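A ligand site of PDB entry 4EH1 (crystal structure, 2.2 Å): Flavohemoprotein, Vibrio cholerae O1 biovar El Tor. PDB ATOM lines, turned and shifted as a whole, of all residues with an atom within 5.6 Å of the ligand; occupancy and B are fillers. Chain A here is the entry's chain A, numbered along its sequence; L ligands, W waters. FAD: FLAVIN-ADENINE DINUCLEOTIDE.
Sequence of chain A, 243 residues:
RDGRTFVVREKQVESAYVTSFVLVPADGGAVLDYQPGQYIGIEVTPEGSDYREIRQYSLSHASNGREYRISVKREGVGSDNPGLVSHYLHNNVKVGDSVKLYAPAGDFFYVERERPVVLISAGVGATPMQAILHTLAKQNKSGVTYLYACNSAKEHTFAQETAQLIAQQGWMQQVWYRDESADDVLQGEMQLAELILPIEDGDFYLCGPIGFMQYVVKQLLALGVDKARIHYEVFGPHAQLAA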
ATOM      1  N   TYR A  39       5.584  12.416  -3.733  1.00  0.00           N
ATOM      2  CA  TYR A  39       5.100  11.333  -4.619  1.00  0.00           C
ATOM      3  C   TYR A  39       6.224  10.364  -4.951  1.00  0.00           C
ATOM      4  O   TYR A  39       7.401  10.722  -4.864  1.00  0.00           O
ATOM      5  CB  TYR A  39       4.537  11.907  -5.951  1.00  0.00           C
ATOM      6  CG  TYR A  39       5.521  12.812  -6.656  1.00  0.00           C
ATOM      7  CD1 TYR A  39       5.500  14.176  -6.443  1.00  0.00           C
ATOM      8  CD2 TYR A  39       6.516  12.286  -7.483  1.00  0.00           C
ATOM      9  CE1 TYR A  39       6.453  15.016  -7.056  1.00  0.00           C
ATOM     10  CE2 TYR A  39       7.453  13.094  -8.084  1.00  0.00           C
ATOM     11  CZ  TYR A  39       7.423  14.458  -7.866  1.00  0.00           C
ATOM     12  OH  TYR A  39       8.348  15.251  -8.488  1.00  0.00           O
ATOM     13  N   ARG A  55       5.183   7.198 -14.401  1.00  0.00           N
ATOM     14  CA  ARG A  55       4.260   8.206 -13.899  1.00  0.00           C
ATOM     15  C   ARG A  55       4.487   8.478 -12.407  1.00  0.00           C
ATOM     16  O   ARG A  55       4.799   7.561 -11.615  1.00  0.00           O
ATOM     17  CB  ARG A  55       2.808   7.723 -14.035  1.00  0.00           C
ATOM     18  CG  ARG A  55       2.395   7.374 -15.494  1.00  0.00           C
ATOM     19  CD  ARG A  55       2.456   8.563 -16.483  1.00  0.00           C
ATOM     20  NE  ARG A  55       1.964   8.167 -17.810  1.00  0.00           N
ATOM     21  CZ  ARG A  55       2.749   7.918 -18.852  1.00  0.00           C
ATOM     22  NH1 ARG A  55       4.066   8.050 -18.730  1.00  0.00           N
ATOM     23  NH2 ARG A  55       2.228   7.546 -20.019  1.00  0.00           N
ATOM     24  N   GLN A  56       4.289   9.739 -12.035  1.00  0.00           N
ATOM     25  CA  GLN A  56       4.258  10.147 -10.630  1.00  0.00           C
ATOM     26  C   GLN A  56       2.942   9.749  -9.987  1.00  0.00           C
ATOM     27  O   GLN A  56       1.868   9.982 -10.561  1.00  0.00           O
ATOM     28  CB  GLN A  56       4.440  11.673 -10.529  1.00  0.00           C
ATOM     29  CG  GLN A  56       5.665  12.215 -11.240  1.00  0.00           C
ATOM     30  CD  GLN A  56       5.345  12.762 -12.624  1.00  0.00           C
ATOM     31  OE1 GLN A  56       4.682  12.104 -13.430  1.00  0.00           O
ATOM     32  NE2 GLN A  56       5.808  13.958 -12.886  1.00  0.00           N
ATOM     33  N   TYR A  57       3.011   9.133  -8.801  1.00  0.00           N
ATOM     34  CA  TYR A  57       1.808   8.954  -7.968  1.00  0.00           C
ATOM     35  C   TYR A  57       2.093   9.361  -6.520  1.00  0.00           C
ATOM     36  O   TYR A  57       3.130   8.990  -5.949  1.00  0.00           O
ATOM     37  CB  TYR A  57       1.251   7.533  -8.034  1.00  0.00           C
ATOM     38  CG  TYR A  57       0.739   7.204  -9.380  1.00  0.00           C
ATOM     39  CD1 TYR A  57      -0.433   7.820  -9.868  1.00  0.00           C
ATOM     40  CD2 TYR A  57       1.439   6.345 -10.226  1.00  0.00           C
ATOM     41  CE1 TYR A  57      -0.896   7.568 -11.164  1.00  0.00           C
ATOM     42  CE2 TYR A  57       0.995   6.099 -11.507  1.00  0.00           C
ATOM     43  CZ  TYR A  57      -0.177   6.710 -11.973  1.00  0.00           C
ATOM     44  OH  TYR A  57      -0.626   6.452 -13.243  1.00  0.00           O
ATOM     45  N   SER A  58       1.175  10.129  -5.940  1.00  0.00           N
ATOM     46  CA  SER A  58       1.333  10.697  -4.629  1.00  0.00           C
ATOM     47  C   SER A  58       1.152   9.640  -3.570  1.00  0.00           C
ATOM     48  O   SER A  58       0.283   8.783  -3.683  1.00  0.00           O
ATOM     49  CB  SER A  58       0.261  11.760  -4.393  1.00  0.00           C
ATOM     50  OG  SER A  58       0.376  12.837  -5.299  1.00  0.00           O
ATOM     51  N   SER A  71      -2.797   6.110  -4.692  1.00  0.00           N
ATOM     52  CA  SER A  71      -4.209   6.070  -5.087  1.00  0.00           C
ATOM     53  C   SER A  71      -4.333   6.649  -6.484  1.00  0.00           C
ATOM     54  O   SER A  71      -4.027   7.837  -6.724  1.00  0.00           O
ATOM     55  CB  SER A  71      -5.066   6.859  -4.107  1.00  0.00           C
ATOM     56  OG  SER A  71      -4.799   6.468  -2.762  1.00  0.00           O
ATOM     57  N   VAL A  72      -4.845   5.818  -7.387  1.00  0.00           N
ATOM     58  CA  VAL A  72      -4.676   6.011  -8.798  1.00  0.00           C
ATOM     59  C   VAL A  72      -6.026   6.176  -9.510  1.00  0.00           C
ATOM     60  O   VAL A  72      -6.895   5.317  -9.452  1.00  0.00           O
ATOM     61  CB  VAL A  72      -3.935   4.792  -9.384  1.00  0.00           C
ATOM     62  CG1 VAL A  72      -3.920   4.857 -10.896  1.00  0.00           C
ATOM     63  CG2 VAL A  72      -2.494   4.654  -8.758  1.00  0.00           C
ATOM     64  N   LYS A  73      -6.194   7.317 -10.161  1.00  0.00           N
ATOM     65  CA  LYS A  73      -7.417   7.547 -10.912  1.00  0.00           C
ATOM     66  C   LYS A  73      -7.322   6.984 -12.341  1.00  0.00           C
ATOM     67  O   LYS A  73      -6.394   7.307 -13.078  1.00  0.00           O
ATOM     68  CB  LYS A  73      -7.744   9.018 -10.987  1.00  0.00           C
ATOM     69  CG  LYS A  73      -9.122   9.210 -11.666  1.00  0.00           C
ATOM     70  CD  LYS A  73      -9.465  10.640 -12.008  1.00  0.00           C
ATOM     71  CE  LYS A  73     -10.584  10.641 -13.075  1.00  0.00           C
ATOM     72  NZ  LYS A  73     -11.116  11.978 -13.410  1.00  0.00           N
ATOM     73  N   GLU A  75      -7.665   7.299 -15.715  1.00  0.00           N
ATOM     74  CA  GLU A  75      -7.817   8.543 -16.488  1.00  0.00           C
ATOM     75  C   GLU A  75      -8.426   8.334 -17.870  1.00  0.00           C
ATOM     76  O   GLU A  75      -8.269   7.294 -18.479  1.00  0.00           O
ATOM     77  CB  GLU A  75      -6.516   9.358 -16.562  1.00  0.00           C
ATOM     78  CG  GLU A  75      -6.747  10.796 -17.121  1.00  0.00           C
ATOM     79  CD  GLU A  75      -5.572  11.757 -16.921  1.00  0.00           C
ATOM     80  OE1 GLU A  75      -5.085  11.890 -15.771  1.00  0.00           O
ATOM     81  OE2 GLU A  75      -5.158  12.398 -17.914  1.00  0.00           O
ATOM     82  N   GLY A  76      -9.185   9.329 -18.331  1.00  0.00           N
ATOM     83  CA  GLY A  76      -9.711   9.310 -19.687  1.00  0.00           C
ATOM     84  C   GLY A  76     -10.724   8.219 -19.944  1.00  0.00           C
ATOM     85  O   GLY A  76     -10.803   7.673 -21.037  1.00  0.00           O
ATOM     86  N   SER A  79     -13.054   8.078 -23.182  1.00  0.00           N
ATOM     87  CA  SER A  79     -12.360   8.831 -24.224  1.00  0.00           C
ATOM     88  C   SER A  79     -11.766   7.913 -25.295  1.00  0.00           C
ATOM     89  O   SER A  79     -11.739   6.693 -25.131  1.00  0.00           O
ATOM     90  CB  SER A  79     -11.249   9.695 -23.624  1.00  0.00           C
ATOM     91  OG  SER A  79     -10.032   8.989 -23.503  1.00  0.00           O
ATOM     92  N   ASN A  81      -8.650   8.031 -25.809  1.00  0.00           N
ATOM     93  CA  ASN A  81      -7.315   7.684 -25.317  1.00  0.00           C
ATOM     94  C   ASN A  81      -7.296   7.425 -23.823  1.00  0.00           C
ATOM     95  O   ASN A  81      -6.848   8.266 -23.046  1.00  0.00           O
ATOM     96  CB  ASN A  81      -6.293   8.757 -25.737  1.00  0.00           C
ATOM     97  CG  ASN A  81      -6.230   8.952 -27.266  1.00  0.00           C
ATOM     98  OD1 ASN A  81      -5.537   8.208 -27.955  1.00  0.00           O
ATOM     99  ND2 ASN A  81      -6.970   9.924 -27.777  1.00  0.00           N
ATOM    100  N   PRO A  82      -7.828   6.261 -23.414  1.00  0.00           N
ATOM    101  CA  PRO A  82      -7.799   5.979 -21.965  1.00  0.00           C
ATOM    102  C   PRO A  82      -6.346   5.949 -21.492  1.00  0.00           C
ATOM    103  O   PRO A  82      -5.504   5.442 -22.224  1.00  0.00           O
ATOM    104  CB  PRO A  82      -8.463   4.607 -21.849  1.00  0.00           C
ATOM    105  CG  PRO A  82      -8.501   4.061 -23.297  1.00  0.00           C
ATOM    106  CD  PRO A  82      -8.529   5.234 -24.197  1.00  0.00           C
ATOM    107  N   GLY A  83      -6.066   6.509 -20.316  1.00  0.00           N
ATOM    108  CA  GLY A  83      -4.679   6.734 -19.909  1.00  0.00           C
ATOM    109  C   GLY A  83      -4.004   5.391 -19.731  1.00  0.00           C
ATOM    110  O   GLY A  83      -4.538   4.493 -19.049  1.00  0.00           O
ATOM    111  N   LEU A  84      -2.831   5.264 -20.334  1.00  0.00           N
ATOM    112  CA  LEU A  84      -2.128   3.994 -20.452  1.00  0.00           C
ATOM    113  C   LEU A  84      -1.737   3.368 -19.124  1.00  0.00           C
ATOM    114  O   LEU A  84      -2.079   2.212 -18.869  1.00  0.00           O
ATOM    115  CB  LEU A  84      -0.862   4.173 -21.272  1.00  0.00           C
ATOM    116  CG  LEU A  84      -0.862   3.598 -22.689  1.00  0.00           C
ATOM    117  CD1 LEU A  84      -2.090   4.040 -23.478  1.00  0.00           C
ATOM    118  CD2 LEU A  84       0.401   4.063 -23.392  1.00  0.00           C
ATOM    119  N   VAL A  85      -1.023   4.117 -18.288  1.00  0.00           N
ATOM    120  CA  VAL A  85      -0.512   3.575 -17.036  1.00  0.00           C
ATOM    121  C   VAL A  85      -1.628   3.376 -16.034  1.00  0.00           C
ATOM    122  O   VAL A  85      -1.679   2.324 -15.352  1.00  0.00           O
ATOM    123  CB  VAL A  85       0.582   4.448 -16.425  1.00  0.00           C
ATOM    124  CG1 VAL A  85       0.919   3.971 -14.987  1.00  0.00           C
ATOM    125  CG2 VAL A  85       1.829   4.460 -17.321  1.00  0.00           C
ATOM    126  N   SER A  86      -2.532   4.357 -15.951  1.00  0.00           N
ATOM    127  CA  SER A  86      -3.634   4.252 -14.968  1.00  0.00           C
ATOM    128  C   SER A  86      -4.522   3.036 -15.285  1.00  0.00           C
ATOM    129  O   SER A  86      -4.926   2.307 -14.377  1.00  0.00           O
ATOM    130  CB  SER A  86      -4.450   5.552 -14.831  1.00  0.00           C
ATOM    131  OG  SER A  86      -5.053   5.974 -16.041  1.00  0.00           O
ATOM    132  N   HIS A  87      -4.774   2.779 -16.564  1.00  0.00           N
ATOM    133  CA  HIS A  87      -5.632   1.647 -16.911  1.00  0.00           C
ATOM    134  C   HIS A  87      -4.869   0.359 -16.696  1.00  0.00           C
ATOM    135  O   HIS A  87      -5.427  -0.653 -16.318  1.00  0.00           O
ATOM    136  CB  HIS A  87      -6.204   1.769 -18.337  1.00  0.00           C
ATOM    137  CG  HIS A  87      -7.333   2.745 -18.426  1.00  0.00           C
ATOM    138  ND1 HIS A  87      -8.646   2.356 -18.600  1.00  0.00           N
ATOM    139  CD2 HIS A  87      -7.353   4.090 -18.276  1.00  0.00           C
ATOM    140  CE1 HIS A  87      -9.426   3.419 -18.584  1.00  0.00           C
ATOM    141  NE2 HIS A  87      -8.664   4.489 -18.399  1.00  0.00           N
ATOM    142  N   VAL A 124      -8.896  13.753  -7.623  1.00  0.00           N
ATOM    143  CA  VAL A 124      -7.796  12.892  -7.203  1.00  0.00           C
ATOM    144  C   VAL A 124      -6.713  13.720  -6.505  1.00  0.00           C
ATOM    145  O   VAL A 124      -5.761  13.172  -5.921  1.00  0.00           O
ATOM    146  CB  VAL A 124      -7.254  12.064  -8.398  1.00  0.00           C
ATOM    147  CG1 VAL A 124      -6.343  12.918  -9.286  1.00  0.00           C
ATOM    148  CG2 VAL A 124      -6.571  10.759  -7.880  1.00  0.00           C
ATOM    149  N   THR A 127      -5.463  12.774  -2.958  1.00  0.00           N
ATOM    150  CA  THR A 127      -4.467  11.752  -2.603  1.00  0.00           C
ATOM    151  C   THR A 127      -3.337  12.287  -1.677  1.00  0.00           C
ATOM    152  O   THR A 127      -3.159  11.776  -0.568  1.00  0.00           O
ATOM    153  CB  THR A 127      -3.912  11.026  -3.861  1.00  0.00           C
ATOM    154  OG1 THR A 127      -4.995  10.477  -4.630  1.00  0.00           O
ATOM    155  CG2 THR A 127      -2.969   9.913  -3.477  1.00  0.00           C
ATOM    156  N   PRO A 128      -2.596  13.339  -2.095  1.00  0.00           N
ATOM    157  CA  PRO A 128      -1.575  13.808  -1.140  1.00  0.00           C
ATOM    158  C   PRO A 128      -2.166  14.402   0.138  1.00  0.00           C
ATOM    159  O   PRO A 128      -1.520  14.302   1.185  1.00  0.00           O
ATOM    160  CB  PRO A 128      -0.828  14.878  -1.937  1.00  0.00           C
ATOM    161  CG  PRO A 128      -1.839  15.317  -3.000  1.00  0.00           C
ATOM    162  CD  PRO A 128      -2.551  14.081  -3.367  1.00  0.00           C
ATOM    163  N   GLU A 233       0.133  21.967  -5.308  1.00  0.00           N
ATOM    164  CA  GLU A 233       0.666  21.051  -6.300  1.00  0.00           C
ATOM    165  C   GLU A 233      -0.404  20.792  -7.375  1.00  0.00           C
ATOM    166  O   GLU A 233      -1.547  20.487  -7.052  1.00  0.00           O
ATOM    167  CB  GLU A 233       1.069  19.741  -5.650  1.00  0.00           C
ATOM    168  CG  GLU A 233       1.824  18.839  -6.628  1.00  0.00           C
ATOM    169  CD  GLU A 233       2.478  17.641  -5.954  1.00  0.00           C
ATOM    170  OE1 GLU A 233       3.725  17.566  -5.938  1.00  0.00           O
ATOM    171  OE2 GLU A 233       1.742  16.783  -5.422  1.00  0.00           O
ATOM    172  N   VAL A 234      -0.022  20.914  -8.637  1.00  0.00           N
ATOM    173  CA  VAL A 234      -0.960  20.678  -9.740  1.00  0.00           C
ATOM    174  C   VAL A 234      -0.773  19.327 -10.393  1.00  0.00           C
ATOM    175  O   VAL A 234       0.348  18.944 -10.744  1.00  0.00           O
ATOM    176  CB  VAL A 234      -0.881  21.791 -10.825  1.00  0.00           C
ATOM    177  CG1 VAL A 234      -1.755  21.452 -12.021  1.00  0.00           C
ATOM    178  CG2 VAL A 234      -1.286  23.097 -10.243  1.00  0.00           C
ATOM    179  N   PHE A 235      -1.860  18.582 -10.494  1.00  0.00           N
ATOM    180  CA  PHE A 235      -1.967  17.464 -11.457  1.00  0.00           C
ATOM    181  C   PHE A 235      -3.434  17.235 -11.801  1.00  0.00           C
ATOM    182  O   PHE A 235      -4.311  17.418 -10.956  1.00  0.00           O
ATOM    183  CB  PHE A 235      -1.241  16.198 -11.010  1.00  0.00           C
ATOM    184  CG  PHE A 235      -1.649  15.664  -9.660  1.00  0.00           C
ATOM    185  CD1 PHE A 235      -2.634  14.674  -9.539  1.00  0.00           C
ATOM    186  CD2 PHE A 235      -1.003  16.077  -8.513  1.00  0.00           C
ATOM    187  CE1 PHE A 235      -2.985  14.153  -8.297  1.00  0.00           C
ATOM    188  CE2 PHE A 235      -1.333  15.535  -7.275  1.00  0.00           C
ATOM    189  CZ  PHE A 235      -2.325  14.568  -7.168  1.00  0.00           C
ATOM    190  N   GLY A 236      -3.701  16.860 -13.043  1.00  0.00           N
ATOM    191  CA  GLY A 236      -5.028  17.077 -13.604  1.00  0.00           C
ATOM    192  C   GLY A 236      -5.809  15.916 -14.171  1.00  0.00           C
ATOM    193  O   GLY A 236      -6.077  14.936 -13.474  1.00  0.00           O
ATOM    194  N   PRO A 237      -6.225  16.034 -15.448  1.00  0.00           N
ATOM    195  CA  PRO A 237      -5.926  17.174 -16.306  1.00  0.00           C
ATOM    196  C   PRO A 237      -7.027  18.223 -16.255  1.00  0.00           C
ATOM    197  O   PRO A 237      -6.731  19.382 -16.554  1.00  0.00           O
ATOM    198  CB  PRO A 237      -5.873  16.548 -17.706  1.00  0.00           C
ATOM    199  CG  PRO A 237      -6.516  15.160 -17.569  1.00  0.00           C
ATOM    200  CD  PRO A 237      -7.024  15.035 -16.161  1.00  0.00           C
HETATM  201  PA  FAD L   1      -1.639   8.944 -20.351  1.00  0.00           P
HETATM  202  O1A FAD L   1      -0.387   9.584 -20.062  1.00  0.00           O
HETATM  203  O2A FAD L   1      -1.740   7.817 -21.216  1.00  0.00           O
HETATM  204  O5B FAD L   1      -2.555  10.026 -20.964  1.00  0.00           O
HETATM  205  C5B FAD L   1      -2.452  11.365 -20.578  1.00  0.00           C
HETATM  206  C4B FAD L   1      -3.544  12.254 -21.157  1.00  0.00           C
HETATM  207  O4B FAD L   1      -3.333  12.497 -22.532  1.00  0.00           O
HETATM  208  C3B FAD L   1      -4.871  11.565 -21.028  1.00  0.00           C
HETATM  209  O3B FAD L   1      -5.848  12.549 -20.803  1.00  0.00           O
HETATM  210  C2B FAD L   1      -5.096  10.971 -22.379  1.00  0.00           C
HETATM  211  O2B FAD L   1      -6.473  10.934 -22.597  1.00  0.00           O
HETATM  212  C1B FAD L   1      -4.358  11.900 -23.297  1.00  0.00           C
HETATM  213  N9A FAD L   1      -3.759  11.117 -24.384  1.00  0.00           N
HETATM  214  C8A FAD L   1      -3.070  10.010 -24.271  1.00  0.00           C
HETATM  215  N7A FAD L   1      -2.697   9.549 -25.473  1.00  0.00           N
HETATM  216  C5A FAD L   1      -3.173  10.388 -26.361  1.00  0.00           C
HETATM  217  C6A FAD L   1      -3.142  10.472 -27.819  1.00  0.00           C
HETATM  218  N6A FAD L   1      -2.500   9.548 -28.559  1.00  0.00           N
HETATM  219  N1A FAD L   1      -3.775  11.489 -28.363  1.00  0.00           N
HETATM  220  C2A FAD L   1      -4.391  12.403 -27.639  1.00  0.00           C
HETATM  221  N3A FAD L   1      -4.464  12.382 -26.328  1.00  0.00           N
HETATM  222  C4A FAD L   1      -3.890  11.415 -25.638  1.00  0.00           C
HETATM  223  N1  FAD L   1      -2.361  10.545 -10.596  1.00  0.00           N
HETATM  224  C2  FAD L   1      -3.055   9.830  -9.706  1.00  0.00           C
HETATM  225  O2  FAD L   1      -3.920   9.089 -10.117  1.00  0.00           O
HETATM  226  N3  FAD L   1      -2.832   9.852  -8.412  1.00  0.00           N
HETATM  227  C4  FAD L   1      -1.906  10.596  -7.883  1.00  0.00           C
HETATM  228  O4  FAD L   1      -1.757  10.572  -6.687  1.00  0.00           O
HETATM  229  C4X FAD L   1      -1.114  11.434  -8.782  1.00  0.00           C
HETATM  230  N5  FAD L   1      -0.166  12.233  -8.343  1.00  0.00           N
HETATM  231  C5X FAD L   1       0.530  12.986  -9.166  1.00  0.00           C
HETATM  232  C6  FAD L   1       1.497  13.787  -8.645  1.00  0.00           C
HETATM  233  C7  FAD L   1       2.229  14.587  -9.464  1.00  0.00           C
HETATM  234  C7M FAD L   1       3.275  15.475  -8.904  1.00  0.00           C
HETATM  235  C8  FAD L   1       1.998  14.562 -10.905  1.00  0.00           C
HETATM  236  C8M FAD L   1       2.831  15.441 -11.770  1.00  0.00           C
HETATM  237  C9  FAD L   1       1.038  13.751 -11.433  1.00  0.00           C
HETATM  238  C9A FAD L   1       0.285  12.963 -10.611  1.00  0.00           C
HETATM  239  N10 FAD L   1      -0.699  12.140 -11.118  1.00  0.00           N
HETATM  240  C10 FAD L   1      -1.417  11.363 -10.208  1.00  0.00           C
HETATM  241  C1' FAD L   1      -0.940  12.065 -12.555  1.00  0.00           C
HETATM  242  C2' FAD L   1      -0.327  10.771 -13.104  1.00  0.00           C
HETATM  243  O2' FAD L   1       1.074  10.722 -12.989  1.00  0.00           O
HETATM  244  C3' FAD L   1      -0.567  10.498 -14.577  1.00  0.00           C
HETATM  245  O3' FAD L   1      -0.234  11.601 -15.370  1.00  0.00           O
HETATM  246  C4' FAD L   1      -1.951   9.972 -14.909  1.00  0.00           C
HETATM  247  O4' FAD L   1      -2.182   8.810 -14.137  1.00  0.00           O
HETATM  248  C5' FAD L   1      -2.163   9.667 -16.393  1.00  0.00           C
HETATM  249  O5' FAD L   1      -1.314   8.689 -16.907  1.00  0.00           O
HETATM  250  P   FAD L   1      -1.755   7.627 -17.926  1.00  0.00           P
HETATM  251  O1P FAD L   1      -0.561   6.963 -18.347  1.00  0.00           O
HETATM  252  O2P FAD L   1      -2.778   6.851 -17.341  1.00  0.00           O
HETATM  253  O3P FAD L   1      -2.354   8.494 -19.053  1.00  0.00           O
HETATM  254  O   HOH W   1      -1.707   8.316  -5.633  1.00  0.00           O
HETATM  255  O   HOH W   2      -2.392  13.437 -15.525  1.00  0.00           O
HETATM  256  O   HOH W   3      -4.449   9.115 -12.866  1.00  0.00           O
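An oxygen (O2') of the ligand sits at hydrogen-bond distance from the backbone NH (N) of Gln 56, at 3.5 Å.
An oxygen (O2') of the ligand lies within hydrogen-bond range of the backbone carbonyl oxygen of Gln 56, at 2.7 Å.
The backbone carbonyl oxygen (O) of Asn 81 lies within hydrogen-bond range of an oxygen (O2B) of the ligand, at 2.7 Å.
The side-chain amide oxygen of Asn 81 sits close to a nitrogen (N6A) of the ligand, 3.4 Å away.
N of Ser 86 is in hydrogen-bond range of O2P of the ligand (2.9 Å).
The side-chain hydroxyl (OG) of Ser 86 sits at hydrogen-bond distance from an oxygen (O2P) of the ligand.
The guanidinium group (NE) of Arg 55 is in salt-bridge range of an oxygen (O1P) of the ligand (2.8 Å).
An oxygen (O1P) of the ligand is in hydrogen-bond range of the backbone NH (N) of Val 85, 2.9 Å away.
N of Lys 73 is in hydrogen-bond range of O2 of the ligand, 2.9 Å away.
O of Ser 71 sits at hydrogen-bond distance from N3 of the ligand (2.9 Å).
The backbone NH (N) of Leu 84 lies within hydrogen-bond range of an oxygen (O2A) of the ligand (2.9 Å).
OH of Tyr 57 is in hydrogen-bond range of O4' of the ligand (3.0 Å).
The side-chain carboxylate (OE2) of Glu 75 sits at hydrogen-bond distance from an oxygen (O3B) of the ligand (3.0 Å).
O4 of the ligand sits at hydrogen-bond distance from N of Ser 58.
The side-chain hydroxyl (OG) of Ser 58 lies within hydrogen-bond range of a nitrogen (N5) of the ligand.
The backbone NH of Asn 81 sits at hydrogen-bond distance from the side-chain hydroxyl of Ser 79 (2.9 Å).
The side-chain hydroxyl (OG) of Ser 86 sits at hydrogen-bond distance from the backbone NH (N) of Glu 75 (2.9 Å).
OG of Ser 86 lies within hydrogen-bond range of O of Gly 83 (3.4 Å).
The backbone carbonyl oxygen (O) of Glu 75 is in hydrogen-bond range of the backbone NH (N) of Gly 83, 3.0 Å away.
The backbone carbonyl oxygen of Glu 75 lies within hydrogen-bond range of a ring nitrogen (NE2) of His 87, at 2.8 Å.
The backbone carbonyl oxygen (O) of Val 124 sits at hydrogen-bond distance from the side-chain hydroxyl (OG1) of Thr 127, 3.1 Å away.
The backbone carbonyl oxygen of Gly 83 lies close to an oxygen (O2P) of the ligand, 3.4 Å away.
Merely in contact with the ligand: Phe 235, Val 72, Thr 127, Tyr 39, Glu 233 and Val 124.
Hydrophobic or aromatic side chains within 4 Å of the ligand: Tyr 39, Tyr 57, Leu 84, Val 85, Val 124 and Phe 235.
Water W3 bridges an oxygen (O4') of the ligand (2.6 Å) and the backbone carbonyl oxygen of Lys 73 (2.7 Å).
Water W2 lies within hydrogen-bond range of O3' of the ligand and OE1 of Glu 75.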
